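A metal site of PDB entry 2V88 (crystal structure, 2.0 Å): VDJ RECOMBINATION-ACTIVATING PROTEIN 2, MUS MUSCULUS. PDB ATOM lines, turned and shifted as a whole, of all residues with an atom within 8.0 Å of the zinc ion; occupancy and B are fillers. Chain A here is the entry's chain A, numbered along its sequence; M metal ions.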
ATOM      1  N   CYS A  14       1.408  -8.348  14.802  1.00  0.00           N
ATOM      2  CA  CYS A  14       2.550  -7.997  13.963  1.00  0.00           C
ATOM      3  C   CYS A  14       2.514  -6.708  13.156  1.00  0.00           C
ATOM      4  O   CYS A  14       3.562  -6.186  12.786  1.00  0.00           O
ATOM      5  CB  CYS A  14       2.899  -9.160  13.023  1.00  0.00           C
ATOM      6  SG  CYS A  14       1.947  -9.249  11.484  1.00  0.00           S
ATOM      7  N   CYS A  15       1.328  -6.214  12.852  1.00  0.00           N
ATOM      8  CA  CYS A  15       1.187  -4.988  12.079  1.00  0.00           C
ATOM      9  C   CYS A  15      -0.229  -4.429  12.257  1.00  0.00           C
ATOM     10  O   CYS A  15      -1.078  -5.051  12.870  1.00  0.00           O
ATOM     11  CB  CYS A  15       1.471  -5.266  10.595  1.00  0.00           C
ATOM     12  SG  CYS A  15       0.311  -6.396   9.814  1.00  0.00           S
ATOM     13  N   ILE A  39       8.244 -14.433   9.661  1.00  0.00           N
ATOM     14  CA  ILE A  39       9.440 -14.026   8.952  1.00  0.00           C
ATOM     15  C   ILE A  39       9.959 -12.732   9.573  1.00  0.00           C
ATOM     16  O   ILE A  39       9.203 -11.876   9.999  1.00  0.00           O
ATOM     17  CB  ILE A  39       9.156 -13.851   7.442  1.00  0.00           C
ATOM     18  CG1 ILE A  39      10.457 -13.458   6.702  1.00  0.00           C
ATOM     19  CG2 ILE A  39       8.052 -12.838   7.220  1.00  0.00           C
ATOM     20  CD1 ILE A  39      10.373 -13.570   5.186  1.00  0.00           C
ATOM     21  N   TYR A  40      11.281 -12.612   9.615  1.00  0.00           N
ATOM     22  CA  TYR A  40      11.929 -11.473  10.228  1.00  0.00           C
ATOM     23  C   TYR A  40      12.117 -10.289   9.276  1.00  0.00           C
ATOM     24  O   TYR A  40      12.691 -10.437   8.203  1.00  0.00           O
ATOM     25  CB  TYR A  40      13.289 -11.928  10.765  1.00  0.00           C
ATOM     26  CG  TYR A  40      14.009 -10.927  11.629  1.00  0.00           C
ATOM     27  CD1 TYR A  40      13.594 -10.679  12.938  1.00  0.00           C
ATOM     28  CD2 TYR A  40      15.125 -10.249  11.145  1.00  0.00           C
ATOM     29  CE1 TYR A  40      14.273  -9.778  13.752  1.00  0.00           C
ATOM     30  CE2 TYR A  40      15.816  -9.349  11.952  1.00  0.00           C
ATOM     31  CZ  TYR A  40      15.387  -9.115  13.251  1.00  0.00           C
ATOM     32  OH  TYR A  40      16.083  -8.238  14.055  1.00  0.00           O
ATOM     33  N   CYS A  41      11.622  -9.118   9.668  1.00  0.00           N
ATOM     34  CA  CYS A  41      11.780  -7.901   8.871  1.00  0.00           C
ATOM     35  C   CYS A  41      13.054  -7.238   9.385  1.00  0.00           C
ATOM     36  O   CYS A  41      13.185  -6.980  10.586  1.00  0.00           O
ATOM     37  CB  CYS A  41      10.599  -6.945   9.077  1.00  0.00           C
ATOM     38  SG  CYS A  41      10.903  -5.272   8.460  1.00  0.00           S
ATOM     39  N   SER A  42      13.979  -6.940   8.475  1.00  0.00           N
ATOM     40  CA  SER A  42      15.255  -6.347   8.857  1.00  0.00           C
ATOM     41  C   SER A  42      15.281  -4.834   9.054  1.00  0.00           C
ATOM     42  O   SER A  42      16.341  -4.264   9.283  1.00  0.00           O
ATOM     43  CB  SER A  42      16.331  -6.756   7.838  1.00  0.00           C
ATOM     44  OG  SER A  42      16.556  -8.157   7.878  1.00  0.00           O
ATOM     45  N   HIS A  43      14.125  -4.187   8.972  1.00  0.00           N
ATOM     46  CA  HIS A  43      14.082  -2.734   9.153  1.00  0.00           C
ATOM     47  C   HIS A  43      14.417  -2.311  10.592  1.00  0.00           C
ATOM     48  O   HIS A  43      13.981  -2.942  11.538  1.00  0.00           O
ATOM     49  CB  HIS A  43      12.708  -2.185   8.793  1.00  0.00           C
ATOM     50  CG  HIS A  43      12.569  -0.714   9.049  1.00  0.00           C
ATOM     51  ND1 HIS A  43      13.219   0.235   8.291  1.00  0.00           N
ATOM     52  CD2 HIS A  43      11.897  -0.037   9.998  1.00  0.00           C
ATOM     53  CE1 HIS A  43      12.947   1.432   8.764  1.00  0.00           C
ATOM     54  NE2 HIS A  43      12.146   1.300   9.805  1.00  0.00           N
ATOM     55  N   GLY A  44      15.186  -1.222  10.718  1.00  0.00           N
ATOM     56  CA  GLY A  44      15.554  -0.713  12.027  1.00  0.00           C
ATOM     57  C   GLY A  44      16.224  -1.752  12.904  1.00  0.00           C
ATOM     58  O   GLY A  44      17.207  -2.358  12.513  1.00  0.00           O
ATOM     59  N   GLY A  46      14.843  -4.343  13.670  1.00  0.00           N
ATOM     60  CA  GLY A  46      14.251  -5.597  13.241  1.00  0.00           C
ATOM     61  C   GLY A  46      13.070  -6.038  14.088  1.00  0.00           C
ATOM     62  O   GLY A  46      12.976  -5.695  15.252  1.00  0.00           O
ATOM     63  N   HIS A  47      12.167  -6.813  13.485  1.00  0.00           N
ATOM     64  CA  HIS A  47      11.003  -7.335  14.185  1.00  0.00           C
ATOM     65  C   HIS A  47      10.411  -8.492  13.405  1.00  0.00           C
ATOM     66  O   HIS A  47      10.715  -8.689  12.240  1.00  0.00           O
ATOM     67  CB  HIS A  47       9.933  -6.240  14.389  1.00  0.00           C
ATOM     68  CG  HIS A  47       9.343  -5.716  13.109  1.00  0.00           C
ATOM     69  ND1 HIS A  47       7.983  -5.715  12.870  1.00  0.00           N
ATOM     70  CD2 HIS A  47       9.922  -5.147  12.032  1.00  0.00           C
ATOM     71  CE1 HIS A  47       7.756  -5.161  11.700  1.00  0.00           C
ATOM     72  NE2 HIS A  47       8.905  -4.803  11.163  1.00  0.00           N
ATOM     73  N   TRP A  48       9.566  -9.269  14.074  1.00  0.00           N
ATOM     74  CA  TRP A  48       8.944 -10.420  13.438  1.00  0.00           C
ATOM     75  C   TRP A  48       7.489 -10.138  13.040  1.00  0.00           C
ATOM     76  O   TRP A  48       6.766  -9.469  13.753  1.00  0.00           O
ATOM     77  CB  TRP A  48       8.973 -11.616  14.380  1.00  0.00           C
ATOM     78  CG  TRP A  48      10.326 -12.212  14.598  1.00  0.00           C
ATOM     79  CD1 TRP A  48      11.232 -11.866  15.574  1.00  0.00           C
ATOM     80  CD2 TRP A  48      10.920 -13.280  13.856  1.00  0.00           C
ATOM     81  NE1 TRP A  48      12.350 -12.665  15.477  1.00  0.00           N
ATOM     82  CE2 TRP A  48      12.188 -13.540  14.422  1.00  0.00           C
ATOM     83  CE3 TRP A  48      10.503 -14.041  12.755  1.00  0.00           C
ATOM     84  CZ2 TRP A  48      13.035 -14.527  13.935  1.00  0.00           C
ATOM     85  CZ3 TRP A  48      11.350 -15.028  12.267  1.00  0.00           C
ATOM     86  CH2 TRP A  48      12.600 -15.266  12.858  1.00  0.00           C
ATOM     87  N   VAL A  49       7.085 -10.666  11.894  1.00  0.00           N
ATOM     88  CA  VAL A  49       5.709 -10.512  11.427  1.00  0.00           C
ATOM     89  C   VAL A  49       5.203 -11.855  10.927  1.00  0.00           C
ATOM     90  O   VAL A  49       5.992 -12.735  10.598  1.00  0.00           O
ATOM     91  CB  VAL A  49       5.592  -9.476  10.276  1.00  0.00           C
ATOM     92  CG1 VAL A  49       5.975  -8.089  10.775  1.00  0.00           C
ATOM     93  CG2 VAL A  49       6.459  -9.882   9.086  1.00  0.00           C
ATOM     94  N   MET A  54       1.394 -10.677   5.657  1.00  0.00           N
ATOM     95  CA  MET A  54       2.138  -9.931   4.641  1.00  0.00           C
ATOM     96  C   MET A  54       1.640 -10.349   3.260  1.00  0.00           C
ATOM     97  O   MET A  54       2.136  -9.867   2.242  1.00  0.00           O
ATOM     98  CB  MET A  54       3.627 -10.224   4.766  1.00  0.00           C
ATOM     99  CG  MET A  54       4.238  -9.827   6.114  1.00  0.00           C
ATOM    100  SD  MET A  54       4.157  -8.039   6.408  1.00  0.00           S
ATOM    101  CE  MET A  54       2.861  -7.938   7.627  1.00  0.00           C
ATOM    102  N   TYR A  71      14.429  -9.635   4.427  1.00  0.00           N
ATOM    103  CA  TYR A  71      13.045  -9.316   4.120  1.00  0.00           C
ATOM    104  C   TYR A  71      12.614  -8.046   4.833  1.00  0.00           C
ATOM    105  O   TYR A  71      13.084  -7.756   5.938  1.00  0.00           O
ATOM    106  CB  TYR A  71      12.137 -10.491   4.539  1.00  0.00           C
ATOM    107  CG  TYR A  71      10.662 -10.178   4.395  1.00  0.00           C
ATOM    108  CD1 TYR A  71       9.897  -9.797   5.510  1.00  0.00           C
ATOM    109  CD2 TYR A  71      10.031 -10.237   3.160  1.00  0.00           C
ATOM    110  CE1 TYR A  71       8.550  -9.477   5.374  1.00  0.00           C
ATOM    111  CE2 TYR A  71       8.689  -9.912   3.018  1.00  0.00           C
ATOM    112  CZ  TYR A  71       7.961  -9.533   4.124  1.00  0.00           C
ATOM    113  OH  TYR A  71       6.637  -9.185   3.971  1.00  0.00           O
ATOM    114  N   TYR A  72      11.722  -7.291   4.194  1.00  0.00           N
ATOM    115  CA  TYR A  72      11.192  -6.067   4.773  1.00  0.00           C
ATOM    116  C   TYR A  72       9.681  -6.103   4.672  1.00  0.00           C
ATOM    117  O   TYR A  72       9.131  -6.170   3.585  1.00  0.00           O
ATOM    118  CB  TYR A  72      11.740  -4.829   4.049  1.00  0.00           C
ATOM    119  CG  TYR A  72      13.236  -4.707   4.177  1.00  0.00           C
ATOM    120  CD1 TYR A  72      14.090  -5.388   3.312  1.00  0.00           C
ATOM    121  CD2 TYR A  72      13.801  -3.934   5.194  1.00  0.00           C
ATOM    122  CE1 TYR A  72      15.466  -5.313   3.462  1.00  0.00           C
ATOM    123  CE2 TYR A  72      15.182  -3.855   5.352  1.00  0.00           C
ATOM    124  CZ  TYR A  72      16.010  -4.550   4.485  1.00  0.00           C
ATOM    125  OH  TYR A  72      17.369  -4.479   4.634  1.00  0.00           O
ATOM    126  N   CYS A  73       9.008  -6.078   5.820  1.00  0.00           N
ATOM    127  CA  CYS A  73       7.547  -6.136   5.830  1.00  0.00           C
ATOM    128  C   CYS A  73       6.924  -5.045   4.961  1.00  0.00           C
ATOM    129  O   CYS A  73       7.595  -4.107   4.544  1.00  0.00           O
ATOM    130  CB  CYS A  73       7.005  -6.050   7.266  1.00  0.00           C
ATOM    131  SG  CYS A  73       7.110  -4.408   8.017  1.00  0.00           S
ATOM    132  N   ASN A  74       5.632  -5.189   4.693  1.00  0.00           N
ATOM    133  CA  ASN A  74       4.901  -4.252   3.845  1.00  0.00           C
ATOM    134  C   ASN A  74       4.950  -2.807   4.375  1.00  0.00           C
ATOM    135  O   ASN A  74       4.901  -1.857   3.604  1.00  0.00           O
ATOM    136  CB  ASN A  74       3.467  -4.752   3.677  1.00  0.00           C
ATOM    137  CG  ASN A  74       3.413  -6.060   2.895  1.00  0.00           C
ATOM    138  OD1 ASN A  74       2.474  -6.850   3.034  1.00  0.00           O
ATOM    139  ND2 ASN A  74       4.409  -6.297   2.051  1.00  0.00           N
ATOM    140  N   GLU A  75       4.983  -2.678   5.693  1.00  0.00           N
ATOM    141  CA  GLU A  75       5.120  -1.371   6.296  1.00  0.00           C
ATOM    142  C   GLU A  75       6.404  -0.679   6.063  1.00  0.00           C
ATOM    143  O   GLU A  75       6.393   0.462   5.942  1.00  0.00           O
ATOM    144  CB  GLU A  75       5.014  -1.365   7.805  1.00  0.00           C
ATOM    145  CG  GLU A  75       3.884  -1.984   8.304  1.00  0.00           C
ATOM    146  CD  GLU A  75       2.847  -1.057   8.669  1.00  0.00           C
ATOM    147  OE1 GLU A  75       2.902  -0.442   9.737  1.00  0.00           O
ATOM    148  OE2 GLU A  75       1.921  -0.942   7.896  1.00  0.00           O
ATOM    149  N   HIS A  76       7.522  -1.390   6.086  1.00  0.00           N
ATOM    150  CA  HIS A  76       8.822  -0.752   5.939  1.00  0.00           C
ATOM    151  C   HIS A  76       9.533  -0.919   4.598  1.00  0.00           C
ATOM    152  O   HIS A  76      10.521  -0.253   4.341  1.00  0.00           O
ATOM    153  CB  HIS A  76       9.732  -1.282   7.039  1.00  0.00           C
ATOM    154  CG  HIS A  76       9.204  -1.067   8.422  1.00  0.00           C
ATOM    155  ND1 HIS A  76       9.292  -2.034   9.396  1.00  0.00           N
ATOM    156  CD2 HIS A  76       8.598  -0.002   8.991  1.00  0.00           C
ATOM    157  CE1 HIS A  76       8.751  -1.568  10.522  1.00  0.00           C
ATOM    158  NE2 HIS A  76       8.333  -0.341  10.293  1.00  0.00           N
ATOM    159  N   VAL A  77       9.024  -1.806   3.750  1.00  0.00           N
ATOM    160  CA  VAL A  77       9.662  -2.079   2.473  1.00  0.00           C
ATOM    161  C   VAL A  77       9.936  -0.867   1.583  1.00  0.00           C
ATOM    162  O   VAL A  77      10.943  -0.828   0.892  1.00  0.00           O
ATOM    163  CB  VAL A  77       8.873  -3.120   1.661  1.00  0.00           C
ATOM    164  CG1 VAL A  77       7.606  -2.497   1.104  1.00  0.00           C
ATOM    165  CG2 VAL A  77       9.732  -3.686   0.562  1.00  0.00           C
ATOM    166  N   ILE A  79      10.664   2.105   2.574  1.00  0.00           N
ATOM    167  CA  ILE A  79      11.513   3.083   3.241  1.00  0.00           C
ATOM    168  C   ILE A  79      12.928   3.078   2.686  1.00  0.00           C
ATOM    169  O   ILE A  79      13.548   2.024   2.568  1.00  0.00           O
ATOM    170  CB  ILE A  79      11.576   2.840   4.756  1.00  0.00           C
ATOM    171  CG1 ILE A  79      10.191   3.019   5.379  1.00  0.00           C
ATOM    172  CG2 ILE A  79      12.586   3.790   5.405  1.00  0.00           C
ATOM    173  CD1 ILE A  79      10.149   2.873   6.880  1.00  0.00           C
HETATM  174 ZN    ZN M   1       9.051  -4.172   9.231  1.00  0.00          ZN
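The backbone NH (N) of His 43 lies close to the side-chain sulfur (SG) of Cys 41, at 3.4 Å. The backbone NH of Glu 75 sits close to the side-chain sulfur of Cys 73, at 3.6 Å.
A ring nitrogen (NE2) of His 47 is bound to the zinc ion (2.0 Å). The zinc ion is bound by ND1 of His 76, at 2.2 Å. SG of Cys 41 binds the zinc ion, 2.3 Å away. The zinc ion is bound by SG of Cys 73. The zinc ion has four donor atoms within binding distance.
Four residues have an atom within 4 Å of the zinc ion: Cys 41, His 47, Cys 73 and His 76. The nearest printed residue that does not touch the zinc ion is His 43 (4.2 Å).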
